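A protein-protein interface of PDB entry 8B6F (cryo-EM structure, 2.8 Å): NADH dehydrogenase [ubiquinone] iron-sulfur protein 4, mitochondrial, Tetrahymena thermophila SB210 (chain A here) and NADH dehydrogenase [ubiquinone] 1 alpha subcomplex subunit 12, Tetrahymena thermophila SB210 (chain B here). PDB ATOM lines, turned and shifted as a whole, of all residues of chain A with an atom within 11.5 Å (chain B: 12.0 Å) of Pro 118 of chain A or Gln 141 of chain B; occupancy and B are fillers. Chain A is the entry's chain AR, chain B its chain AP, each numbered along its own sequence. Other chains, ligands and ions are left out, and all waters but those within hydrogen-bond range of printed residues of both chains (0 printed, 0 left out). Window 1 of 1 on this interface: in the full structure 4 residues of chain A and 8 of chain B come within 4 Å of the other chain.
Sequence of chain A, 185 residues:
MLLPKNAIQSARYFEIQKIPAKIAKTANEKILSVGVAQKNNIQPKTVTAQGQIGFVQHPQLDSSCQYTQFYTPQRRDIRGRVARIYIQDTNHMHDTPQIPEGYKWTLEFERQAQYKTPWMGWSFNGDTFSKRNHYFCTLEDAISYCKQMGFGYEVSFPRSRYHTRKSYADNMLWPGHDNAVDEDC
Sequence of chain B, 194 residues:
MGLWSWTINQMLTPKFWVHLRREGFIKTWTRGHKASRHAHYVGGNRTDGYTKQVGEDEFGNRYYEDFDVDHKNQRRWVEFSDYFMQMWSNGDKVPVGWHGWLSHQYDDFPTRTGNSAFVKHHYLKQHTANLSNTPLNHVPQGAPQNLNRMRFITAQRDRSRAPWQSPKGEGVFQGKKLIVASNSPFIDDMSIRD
Of the printed residues of chain B, Lys 116 of chain A touches Gln 156. Trp 119 of chain A touches just these residues of chain B: Pro 140 (3.8 Å), Gln 141 (2.6 Å), Gly 142 (3.8 Å) and Ala 143 (3.9 Å). Of the printed residues of chain B, Met 120 of chain A touches Pro 140 (3.7 Å) and Phe 152 (3.98 Å). Val 139 of chain B touches none of the printed residues of chain A. Gln 141 of chain B touches just these residues of chain A: Pro 118 and Trp 119. Of chain A, only Trp 119 (3.9 Å) comes within 4 Å of Ala 143 of chain B. No residue of chain A comes within 4 Å of Asn 146 of chain B. Of the printed residues of chain A, Phe 152 of chain B touches Pro 118 and Met 120. Ile 153 of chain B touches just one residue of chain A: Pro 118 (3.6 Å). The nearest residue of chain A that does not touch Gln 141 of chain B is Met 120 of chain A (4.3 Å). The nearest printed residue of chain A that does not touch Gln 156 of chain B is Gly 121 of chain A (4.4 Å).
O of Gln 141 of chain B sits close to O of Trp 119 of chain A (2.6 Å).
Lys 116 of chain A touches Gln 156 of chain B. Gln 141 of chain B touches Pro 118 of chain A. Pro 118 of chain A touches Gly 142 of chain B. Pro 118 of chain A touches Arg 149 of chain B (CB to NH2, 3.9 Å). Pro 118 of chain A touches Ile 153 of chain B (CB to CD1, 3.6 Å). Pro 140 of chain B touches Trp 119 of chain A (CB to O, 3.8 Å). O of Gly 142 of chain B touches CA of Trp 119 of chain A (3.8 Å). O of Trp 119 of chain A touches N of Ala 143 of chain B (3.9 Å). Pro 140 of chain B touches Met 120 of chain A (CB to SD, 3.7 Å). CZ of Phe 152 of chain B touches O of Met 120 of chain A, 3.98 Å away.
Of the 11 printed residues of chain A, 4 touch a printed residue of chain B. Hydrophobic or aromatic side chains of chain A within 4 Å of the printed part of chain B: Pro 118 and Met 120. Hydrophobic or aromatic side chains of chain B that line the printed part of chain A: Pro 140, Phe 152 and Ile 153.
The guanidinium group (NE) of Arg 149 of chain B is in hydrogen-bond range of the backbone carbonyl oxygen (O) of Gly 142 of chain B, at 3.3 Å. NZ of Lys 116 of chain A lies within hydrogen-bond range of O of Gly 121 of chain A (2.9 Å).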
ATOM      1  N   GLN A 114      19.812  16.059  18.505  1.00  0.00           N
ATOM      2  CA  GLN A 114      19.061  15.325  19.519  1.00  0.00           C
ATOM      3  C   GLN A 114      18.325  16.347  20.373  1.00  0.00           C
ATOM      4  O   GLN A 114      18.959  17.144  21.071  1.00  0.00           O
ATOM      5  CB  GLN A 114      19.983  14.463  20.379  1.00  0.00           C
ATOM      6  CG  GLN A 114      20.562  13.262  19.660  1.00  0.00           C
ATOM      7  CD  GLN A 114      21.644  12.579  20.467  1.00  0.00           C
ATOM      8  OE1 GLN A 114      22.629  13.203  20.857  1.00  0.00           O
ATOM      9  NE2 GLN A 114      21.462  11.291  20.731  1.00  0.00           N
ATOM     10  N   TYR A 115      16.997  16.328  20.321  1.00  0.00           N
ATOM     11  CA  TYR A 115      16.189  17.357  20.955  1.00  0.00           C
ATOM     12  C   TYR A 115      15.039  16.722  21.721  1.00  0.00           C
ATOM     13  O   TYR A 115      14.509  15.682  21.324  1.00  0.00           O
ATOM     14  CB  TYR A 115      15.640  18.348  19.920  1.00  0.00           C
ATOM     15  CG  TYR A 115      15.037  17.685  18.704  1.00  0.00           C
ATOM     16  CD1 TYR A 115      15.831  17.321  17.625  1.00  0.00           C
ATOM     17  CD2 TYR A 115      13.676  17.432  18.632  1.00  0.00           C
ATOM     18  CE1 TYR A 115      15.286  16.716  16.511  1.00  0.00           C
ATOM     19  CE2 TYR A 115      13.121  16.828  17.523  1.00  0.00           C
ATOM     20  CZ  TYR A 115      13.931  16.473  16.465  1.00  0.00           C
ATOM     21  OH  TYR A 115      13.382  15.873  15.358  1.00  0.00           O
ATOM     22  N   LYS A 116      14.665  17.356  22.827  1.00  0.00           N
ATOM     23  CA  LYS A 116      13.542  16.904  23.635  1.00  0.00           C
ATOM     24  C   LYS A 116      12.293  17.661  23.200  1.00  0.00           C
ATOM     25  O   LYS A 116      12.253  18.894  23.270  1.00  0.00           O
ATOM     26  CB  LYS A 116      13.820  17.121  25.122  1.00  0.00           C
ATOM     27  CG  LYS A 116      15.058  16.393  25.618  1.00  0.00           C
ATOM     28  CD  LYS A 116      15.341  16.691  27.082  1.00  0.00           C
ATOM     29  CE  LYS A 116      14.349  16.011  28.007  1.00  0.00           C
ATOM     30  NZ  LYS A 116      14.403  14.527  27.892  1.00  0.00           N
ATOM     31  N   THR A 117      11.279  16.927  22.754  1.00  0.00           N
ATOM     32  CA  THR A 117      10.074  17.549  22.243  1.00  0.00           C
ATOM     33  C   THR A 117       9.302  18.217  23.380  1.00  0.00           C
ATOM     34  O   THR A 117       9.431  17.828  24.540  1.00  0.00           O
ATOM     35  CB  THR A 117       9.199  16.517  21.544  1.00  0.00           C
ATOM     36  OG1 THR A 117       8.960  15.411  22.423  1.00  0.00           O
ATOM     37  CG2 THR A 117       9.880  16.033  20.278  1.00  0.00           C
ATOM     38  N   PRO A 118       8.487  19.231  23.071  1.00  0.00           N
ATOM     39  CA  PRO A 118       7.833  19.990  24.146  1.00  0.00           C
ATOM     40  C   PRO A 118       6.672  19.257  24.805  1.00  0.00           C
ATOM     41  O   PRO A 118       6.469  19.394  26.015  1.00  0.00           O
ATOM     42  CB  PRO A 118       7.345  21.263  23.436  1.00  0.00           C
ATOM     43  CG  PRO A 118       7.970  21.245  22.075  1.00  0.00           C
ATOM     44  CD  PRO A 118       8.201  19.815  21.750  1.00  0.00           C
ATOM     45  N   TRP A 119       5.904  18.483  24.036  1.00  0.00           N
ATOM     46  CA  TRP A 119       4.643  17.961  24.560  1.00  0.00           C
ATOM     47  C   TRP A 119       4.866  17.028  25.744  1.00  0.00           C
ATOM     48  O   TRP A 119       4.094  17.048  26.709  1.00  0.00           O
ATOM     49  CB  TRP A 119       3.858  17.251  23.456  1.00  0.00           C
ATOM     50  CG  TRP A 119       4.618  16.196  22.718  1.00  0.00           C
ATOM     51  CD1 TRP A 119       4.805  14.900  23.099  1.00  0.00           C
ATOM     52  CD2 TRP A 119       5.276  16.343  21.455  1.00  0.00           C
ATOM     53  NE1 TRP A 119       5.545  14.233  22.154  1.00  0.00           N
ATOM     54  CE2 TRP A 119       5.847  15.097  21.135  1.00  0.00           C
ATOM     55  CE3 TRP A 119       5.440  17.410  20.567  1.00  0.00           C
ATOM     56  CZ2 TRP A 119       6.572  14.888  19.965  1.00  0.00           C
ATOM     57  CZ3 TRP A 119       6.160  17.201  19.405  1.00  0.00           C
ATOM     58  CH2 TRP A 119       6.717  15.949  19.113  1.00  0.00           C
ATOM     59  N   MET A 120       5.907  16.195  25.690  1.00  0.00           N
ATOM     60  CA  MET A 120       6.180  15.243  26.757  1.00  0.00           C
ATOM     61  C   MET A 120       7.638  15.211  27.193  1.00  0.00           C
ATOM     62  O   MET A 120       7.965  14.478  28.132  1.00  0.00           O
ATOM     63  CB  MET A 120       5.760  13.828  26.332  1.00  0.00           C
ATOM     64  CG  MET A 120       4.262  13.576  26.394  1.00  0.00           C
ATOM     65  SD  MET A 120       3.639  13.470  28.083  1.00  0.00           S
ATOM     66  CE  MET A 120       4.297  11.889  28.602  1.00  0.00           C
ATOM     67  N   GLY A 121       8.517  15.980  26.556  1.00  0.00           N
ATOM     68  CA  GLY A 121       9.919  15.936  26.915  1.00  0.00           C
ATOM     69  C   GLY A 121      10.640  14.690  26.462  1.00  0.00           C
ATOM     70  O   GLY A 121      11.683  14.350  27.023  1.00  0.00           O
ATOM     71  N   TRP A 122      10.107  13.992  25.464  1.00  0.00           N
ATOM     72  CA  TRP A 122      10.735  12.783  24.952  1.00  0.00           C
ATOM     73  C   TRP A 122      11.866  13.132  23.994  1.00  0.00           C
ATOM     74  O   TRP A 122      11.777  14.093  23.226  1.00  0.00           O
ATOM     75  CB  TRP A 122       9.701  11.906  24.248  1.00  0.00           C
ATOM     76  CG  TRP A 122       8.628  11.396  25.160  1.00  0.00           C
ATOM     77  CD1 TRP A 122       8.681  11.317  26.521  1.00  0.00           C
ATOM     78  CD2 TRP A 122       7.342  10.899  24.779  1.00  0.00           C
ATOM     79  NE1 TRP A 122       7.508  10.799  27.010  1.00  0.00           N
ATOM     80  CE2 TRP A 122       6.670  10.532  25.961  1.00  0.00           C
ATOM     81  CE3 TRP A 122       6.694  10.724  23.552  1.00  0.00           C
ATOM     82  CZ2 TRP A 122       5.381  10.004  25.953  1.00  0.00           C
ATOM     83  CZ3 TRP A 122       5.414  10.199  23.546  1.00  0.00           C
ATOM     84  CH2 TRP A 122       4.771   9.844  24.739  1.00  0.00           C
ATOM     85  N   SER A 123      12.934  12.341  24.043  1.00  0.00           N
ATOM     86  CA  SER A 123      14.092  12.573  23.194  1.00  0.00           C
ATOM     87  C   SER A 123      13.815  12.095  21.775  1.00  0.00           C
ATOM     88  O   SER A 123      13.223  11.034  21.563  1.00  0.00           O
ATOM     89  CB  SER A 123      15.321  11.858  23.753  1.00  0.00           C
ATOM     90  OG  SER A 123      15.643  12.340  25.045  1.00  0.00           O
ATOM     91  N   PHE A 124      14.254  12.890  20.803  1.00  0.00           N
ATOM     92  CA  PHE A 124      14.082  12.603  19.388  1.00  0.00           C
ATOM     93  C   PHE A 124      15.405  12.822  18.672  1.00  0.00           C
ATOM     94  O   PHE A 124      16.154  13.744  19.005  1.00  0.00           O
ATOM     95  CB  PHE A 124      13.011  13.499  18.754  1.00  0.00           C
ATOM     96  CG  PHE A 124      11.600  13.054  19.018  1.00  0.00           C
ATOM     97  CD1 PHE A 124      11.102  12.995  20.307  1.00  0.00           C
ATOM     98  CD2 PHE A 124      10.758  12.735  17.966  1.00  0.00           C
ATOM     99  CE1 PHE A 124       9.801  12.600  20.545  1.00  0.00           C
ATOM    100  CE2 PHE A 124       9.456  12.341  18.197  1.00  0.00           C
ATOM    101  CZ  PHE A 124       8.976  12.277  19.489  1.00  0.00           C
ATOM    102  N   ASN B 137      -9.926  17.040  31.284  1.00  0.00           N
ATOM    103  CA  ASN B 137      -9.309  15.861  30.696  1.00  0.00           C
ATOM    104  C   ASN B 137      -7.801  15.908  30.904  1.00  0.00           C
ATOM    105  O   ASN B 137      -7.227  16.955  31.216  1.00  0.00           O
ATOM    106  CB  ASN B 137      -9.631  15.753  29.201  1.00  0.00           C
ATOM    107  CG  ASN B 137      -9.173  16.966  28.413  1.00  0.00           C
ATOM    108  OD1 ASN B 137      -8.302  17.717  28.849  1.00  0.00           O
ATOM    109  ND2 ASN B 137      -9.762  17.163  27.241  1.00  0.00           N
ATOM    110  N   HIS B 138      -7.163  14.757  30.730  1.00  0.00           N
ATOM    111  CA  HIS B 138      -5.720  14.672  30.906  1.00  0.00           C
ATOM    112  C   HIS B 138      -5.013  15.545  29.879  1.00  0.00           C
ATOM    113  O   HIS B 138      -5.167  15.348  28.670  1.00  0.00           O
ATOM    114  CB  HIS B 138      -5.259  13.220  30.780  1.00  0.00           C
ATOM    115  CG  HIS B 138      -3.775  13.049  30.886  1.00  0.00           C
ATOM    116  ND1 HIS B 138      -3.042  13.547  31.942  1.00  0.00           N
ATOM    117  CD2 HIS B 138      -2.887  12.433  30.070  1.00  0.00           C
ATOM    118  CE1 HIS B 138      -1.767  13.248  31.770  1.00  0.00           C
ATOM    119  NE2 HIS B 138      -1.646  12.572  30.642  1.00  0.00           N
ATOM    120  N   VAL B 139      -4.242  16.513  30.366  1.00  0.00           N
ATOM    121  CA  VAL B 139      -3.457  17.395  29.508  1.00  0.00           C
ATOM    122  C   VAL B 139      -1.982  17.162  29.814  1.00  0.00           C
ATOM    123  O   VAL B 139      -1.527  17.486  30.920  1.00  0.00           O
ATOM    124  CB  VAL B 139      -3.839  18.868  29.715  1.00  0.00           C
ATOM    125  CG1 VAL B 139      -2.988  19.772  28.833  1.00  0.00           C
ATOM    126  CG2 VAL B 139      -5.316  19.082  29.429  1.00  0.00           C
ATOM    127  N   PRO B 140      -1.202  16.604  28.889  1.00  0.00           N
ATOM    128  CA  PRO B 140       0.224  16.401  29.170  1.00  0.00           C
ATOM    129  C   PRO B 140       0.919  17.717  29.476  1.00  0.00           C
ATOM    130  O   PRO B 140       0.615  18.755  28.887  1.00  0.00           O
ATOM    131  CB  PRO B 140       0.754  15.772  27.876  1.00  0.00           C
ATOM    132  CG  PRO B 140      -0.436  15.180  27.218  1.00  0.00           C
ATOM    133  CD  PRO B 140      -1.584  16.068  27.572  1.00  0.00           C
ATOM    134  N   GLN B 141       1.859  17.667  30.416  1.00  0.00           N
ATOM    135  CA  GLN B 141       2.653  18.847  30.730  1.00  0.00           C
ATOM    136  C   GLN B 141       3.429  19.286  29.497  1.00  0.00           C
ATOM    137  O   GLN B 141       4.067  18.470  28.827  1.00  0.00           O
ATOM    138  CB  GLN B 141       3.617  18.550  31.876  1.00  0.00           C
ATOM    139  CG  GLN B 141       2.945  18.091  33.154  1.00  0.00           C
ATOM    140  CD  GLN B 141       3.942  17.722  34.230  1.00  0.00           C
ATOM    141  OE1 GLN B 141       3.804  16.694  34.892  1.00  0.00           O
ATOM    142  NE2 GLN B 141       4.954  18.563  34.419  1.00  0.00           N
ATOM    143  N   GLY B 142       3.375  20.578  29.196  1.00  0.00           N
ATOM    144  CA  GLY B 142       4.026  21.098  28.016  1.00  0.00           C
ATOM    145  C   GLY B 142       3.216  20.993  26.745  1.00  0.00           C
ATOM    146  O   GLY B 142       3.661  21.491  25.703  1.00  0.00           O
ATOM    147  N   ALA B 143       2.046  20.364  26.791  1.00  0.00           N
ATOM    148  CA  ALA B 143       1.200  20.265  25.619  1.00  0.00           C
ATOM    149  C   ALA B 143       0.635  21.639  25.269  1.00  0.00           C
ATOM    150  O   ALA B 143       0.515  22.510  26.132  1.00  0.00           O
ATOM    151  CB  ALA B 143       0.067  19.274  25.862  1.00  0.00           C
ATOM    152  N   PRO B 144       0.276  21.857  24.002  1.00  0.00           N
ATOM    153  CA  PRO B 144      -0.244  23.179  23.618  1.00  0.00           C
ATOM    154  C   PRO B 144      -1.465  23.603  24.413  1.00  0.00           C
ATOM    155  O   PRO B 144      -1.639  24.802  24.666  1.00  0.00           O
ATOM    156  CB  PRO B 144      -0.561  23.013  22.123  1.00  0.00           C
ATOM    157  CG  PRO B 144      -0.598  21.542  21.883  1.00  0.00           C
ATOM    158  CD  PRO B 144       0.361  20.943  22.851  1.00  0.00           C
ATOM    159  N   GLN B 145      -2.320  22.662  24.814  1.00  0.00           N
ATOM    160  CA  GLN B 145      -3.489  23.024  25.608  1.00  0.00           C
ATOM    161  C   GLN B 145      -3.085  23.577  26.967  1.00  0.00           C
ATOM    162  O   GLN B 145      -3.716  24.510  27.476  1.00  0.00           O
ATOM    163  CB  GLN B 145      -4.409  21.816  25.776  1.00  0.00           C
ATOM    164  CG  GLN B 145      -5.665  22.115  26.581  1.00  0.00           C
ATOM    165  CD  GLN B 145      -6.653  20.968  26.569  1.00  0.00           C
ATOM    166  OE1 GLN B 145      -6.504  20.013  25.811  1.00  0.00           O
ATOM    167  NE2 GLN B 145      -7.673  21.059  27.414  1.00  0.00           N
ATOM    168  N   ASN B 146      -2.043  23.015  27.572  1.00  0.00           N
ATOM    169  CA  ASN B 146      -1.596  23.471  28.882  1.00  0.00           C
ATOM    170  C   ASN B 146      -1.052  24.891  28.777  1.00  0.00           C
ATOM    171  O   ASN B 146      -0.034  25.126  28.117  1.00  0.00           O
ATOM    172  CB  ASN B 146      -0.530  22.526  29.429  1.00  0.00           C
ATOM    173  CG  ASN B 146      -0.131  22.858  30.850  1.00  0.00           C
ATOM    174  OD1 ASN B 146      -0.842  23.569  31.557  1.00  0.00           O
ATOM    175  ND2 ASN B 146       1.014  22.341  31.277  1.00  0.00           N
ATOM    176  N   LEU B 147      -1.727  25.837  29.433  1.00  0.00           N
ATOM    177  CA  LEU B 147      -1.304  27.231  29.375  1.00  0.00           C
ATOM    178  C   LEU B 147       0.038  27.460  30.055  1.00  0.00           C
ATOM    179  O   LEU B 147       0.722  28.436  29.733  1.00  0.00           O
ATOM    180  CB  LEU B 147      -2.367  28.129  30.007  1.00  0.00           C
ATOM    181  CG  LEU B 147      -3.755  28.086  29.360  1.00  0.00           C
ATOM    182  CD1 LEU B 147      -4.719  28.986  30.113  1.00  0.00           C
ATOM    183  CD2 LEU B 147      -3.697  28.479  27.891  1.00  0.00           C
ATOM    184  N   ASN B 148       0.430  26.590  30.986  1.00  0.00           N
ATOM    185  CA  ASN B 148       1.723  26.678  31.652  1.00  0.00           C
ATOM    186  C   ASN B 148       2.758  25.766  31.002  1.00  0.00           C
ATOM    187  O   ASN B 148       3.675  25.284  31.673  1.00  0.00           O
ATOM    188  CB  ASN B 148       1.579  26.346  33.137  1.00  0.00           C
ATOM    189  CG  ASN B 148       0.704  27.338  33.870  1.00  0.00           C
ATOM    190  OD1 ASN B 148       0.615  28.504  33.488  1.00  0.00           O
ATOM    191  ND2 ASN B 148       0.053  26.883  34.932  1.00  0.00           N
ATOM    192  N   ARG B 149       2.621  25.518  29.698  1.00  0.00           N
ATOM    193  CA  ARG B 149       3.587  24.680  29.000  1.00  0.00           C
ATOM    194  C   ARG B 149       4.976  25.302  29.007  1.00  0.00           C
ATOM    195  O   ARG B 149       5.977  24.585  28.897  1.00  0.00           O
ATOM    196  CB  ARG B 149       3.122  24.440  27.564  1.00  0.00           C
ATOM    197  CG  ARG B 149       2.923  25.717  26.763  1.00  0.00           C
ATOM    198  CD  ARG B 149       2.481  25.426  25.340  1.00  0.00           C
ATOM    199  NE  ARG B 149       3.446  24.602  24.624  1.00  0.00           N
ATOM    200  CZ  ARG B 149       3.423  24.383  23.317  1.00  0.00           C
ATOM    201  NH1 ARG B 149       2.504  24.931  22.541  1.00  0.00           N
ATOM    202  NH2 ARG B 149       4.346  23.596  22.775  1.00  0.00           N
ATOM    203  N   MET B 150       5.061  26.628  29.131  1.00  0.00           N
ATOM    204  CA  MET B 150       6.360  27.290  29.080  1.00  0.00           C
ATOM    205  C   MET B 150       7.253  26.847  30.231  1.00  0.00           C
ATOM    206  O   MET B 150       8.452  26.619  30.042  1.00  0.00           O
ATOM    207  CB  MET B 150       6.176  28.807  29.100  1.00  0.00           C
ATOM    208  CG  MET B 150       5.598  29.386  27.817  1.00  0.00           C
ATOM    209  SD  MET B 150       6.685  29.184  26.389  1.00  0.00           S
ATOM    210  CE  MET B 150       5.951  27.758  25.589  1.00  0.00           C
ATOM    211  N   ARG B 151       6.688  26.725  31.433  1.00  0.00           N
ATOM    212  CA  ARG B 151       7.488  26.308  32.580  1.00  0.00           C
ATOM    213  C   ARG B 151       8.076  24.921  32.357  1.00  0.00           C
ATOM    214  O   ARG B 151       9.274  24.699  32.570  1.00  0.00           O
ATOM    215  CB  ARG B 151       6.636  26.335  33.848  1.00  0.00           C
ATOM    216  CG  ARG B 151       7.397  25.942  35.102  1.00  0.00           C
ATOM    217  CD  ARG B 151       6.499  25.944  36.327  1.00  0.00           C
ATOM    218  NE  ARG B 151       7.248  25.638  37.539  1.00  0.00           N
ATOM    219  CZ  ARG B 151       6.714  25.549  38.750  1.00  0.00           C
ATOM    220  NH1 ARG B 151       5.418  25.727  38.949  1.00  0.00           N
ATOM    221  NH2 ARG B 151       7.500  25.277  39.788  1.00  0.00           N
ATOM    222  N   PHE B 152       7.246  23.970  31.928  1.00  0.00           N
ATOM    223  CA  PHE B 152       7.732  22.614  31.702  1.00  0.00           C
ATOM    224  C   PHE B 152       8.782  22.582  30.599  1.00  0.00           C
ATOM    225  O   PHE B 152       9.805  21.900  30.726  1.00  0.00           O
ATOM    226  CB  PHE B 152       6.561  21.693  31.359  1.00  0.00           C
ATOM    227  CG  PHE B 152       6.970  20.281  31.059  1.00  0.00           C
ATOM    228  CD1 PHE B 152       7.181  19.375  32.084  1.00  0.00           C
ATOM    229  CD2 PHE B 152       7.131  19.856  29.750  1.00  0.00           C
ATOM    230  CE1 PHE B 152       7.554  18.073  31.810  1.00  0.00           C
ATOM    231  CE2 PHE B 152       7.503  18.555  29.471  1.00  0.00           C
ATOM    232  CZ  PHE B 152       7.713  17.663  30.502  1.00  0.00           C
ATOM    233  N   ILE B 153       8.546  23.314  29.508  1.00  0.00           N
ATOM    234  CA  ILE B 153       9.492  23.310  28.395  1.00  0.00           C
ATOM    235  C   ILE B 153      10.823  23.908  28.826  1.00  0.00           C
ATOM    236  O   ILE B 153      11.893  23.377  28.505  1.00  0.00           O
ATOM    237  CB  ILE B 153       8.895  24.057  27.187  1.00  0.00           C
ATOM    238  CG1 ILE B 153       7.704  23.276  26.627  1.00  0.00           C
ATOM    239  CG2 ILE B 153       9.947  24.266  26.102  1.00  0.00           C
ATOM    240  CD1 ILE B 153       6.877  24.052  25.630  1.00  0.00           C
ATOM    241  N   THR B 154      10.785  25.024  29.555  1.00  0.00           N
ATOM    242  CA  THR B 154      12.022  25.636  30.024  1.00  0.00           C
ATOM    243  C   THR B 154      12.767  24.712  30.978  1.00  0.00           C
ATOM    244  O   THR B 154      13.995  24.592  30.904  1.00  0.00           O
ATOM    245  CB  THR B 154      11.722  26.974  30.702  1.00  0.00           C
ATOM    246  OG1 THR B 154      11.115  27.865  29.758  1.00  0.00           O
ATOM    247  CG2 THR B 154      12.999  27.608  31.241  1.00  0.00           C
ATOM    248  N   ALA B 155      12.042  24.043  31.875  1.00  0.00           N
ATOM    249  CA  ALA B 155      12.696  23.122  32.799  1.00  0.00           C
ATOM    250  C   ALA B 155      13.353  21.970  32.053  1.00  0.00           C
ATOM    251  O   ALA B 155      14.491  21.597  32.354  1.00  0.00           O
ATOM    252  CB  ALA B 155      11.685  22.596  33.816  1.00  0.00           C
ATOM    253  N   GLN B 156      12.658  21.400  31.068  1.00  0.00           N
ATOM    254  CA  GLN B 156      13.242  20.306  30.299  1.00  0.00           C
ATOM    255  C   GLN B 156      14.478  20.770  29.542  1.00  0.00           C
ATOM    256  O   GLN B 156      15.481  20.049  29.476  1.00  0.00           O
ATOM    257  CB  GLN B 156      12.204  19.734  29.333  1.00  0.00           C
ATOM    258  CG  GLN B 156      11.082  18.979  30.021  1.00  0.00           C
ATOM    259  CD  GLN B 156      11.570  17.723  30.712  1.00  0.00           C
ATOM    260  OE1 GLN B 156      12.574  17.133  30.315  1.00  0.00           O
ATOM    261  NE2 GLN B 156      10.865  17.310  31.758  1.00  0.00           N
ATOM    262  N   ARG B 157      14.426  21.968  28.963  1.00  0.00           N
ATOM    263  CA  ARG B 157      15.585  22.500  28.253  1.00  0.00           C
ATOM    264  C   ARG B 157      16.743  22.747  29.210  1.00  0.00           C
ATOM    265  O   ARG B 157      17.904  22.496  28.866  1.00  0.00           O
ATOM    266  CB  ARG B 157      15.202  23.785  27.518  1.00  0.00           C
ATOM    267  CG  ARG B 157      16.334  24.403  26.707  1.00  0.00           C
ATOM    268  CD  ARG B 157      17.002  25.547  27.451  1.00  0.00           C
ATOM    269  NE  ARG B 157      16.088  26.656  27.696  1.00  0.00           N
ATOM    270  CZ  ARG B 157      15.806  27.610  26.819  1.00  0.00           C
ATOM    271  NH1 ARG B 157      16.345  27.622  25.612  1.00  0.00           N
ATOM    272  NH2 ARG B 157      14.962  28.578  27.164  1.00  0.00           N
ATOM    273  N   ASP B 158      16.451  23.244  30.414  1.00  0.00           N
ATOM    274  CA  ASP B 158      17.512  23.566  31.362  1.00  0.00           C
ATOM    275  C   ASP B 158      18.136  22.317  31.969  1.00  0.00           C
ATOM    276  O   ASP B 158      19.290  22.361  32.410  1.00  0.00           O
ATOM    277  CB  ASP B 158      16.970  24.470  32.468  1.00  0.00           C
ATOM    278  CG  ASP B 158      16.477  25.803  31.941  1.00  0.00           C
ATOM    279  OD1 ASP B 158      16.533  26.012  30.712  1.00  0.00           O
ATOM    280  OD2 ASP B 158      16.036  26.642  32.754  1.00  0.00           O
ATOM    281  N   ARG B 159      17.399  21.204  32.021  1.00  0.00           N
ATOM    282  CA  ARG B 159      17.984  19.968  32.531  1.00  0.00           C
ATOM    283  C   ARG B 159      19.266  19.616  31.792  1.00  0.00           C
ATOM    284  O   ARG B 159      20.204  19.080  32.393  1.00  0.00           O
ATOM    285  CB  ARG B 159      16.984  18.813  32.415  1.00  0.00           C
ATOM    286  CG  ARG B 159      15.839  18.878  33.412  1.00  0.00           C
ATOM    287  CD  ARG B 159      15.077  17.563  33.492  1.00  0.00           C
ATOM    288  NE  ARG B 159      15.718  16.611  34.395  1.00  0.00           N
ATOM    289  CZ  ARG B 159      16.563  15.657  34.023  1.00  0.00           C
ATOM    290  NH1 ARG B 159      16.903  15.486  32.756  1.00  0.00           N
ATOM    291  NH2 ARG B 159      17.078  14.853  34.948  1.00  0.00           N
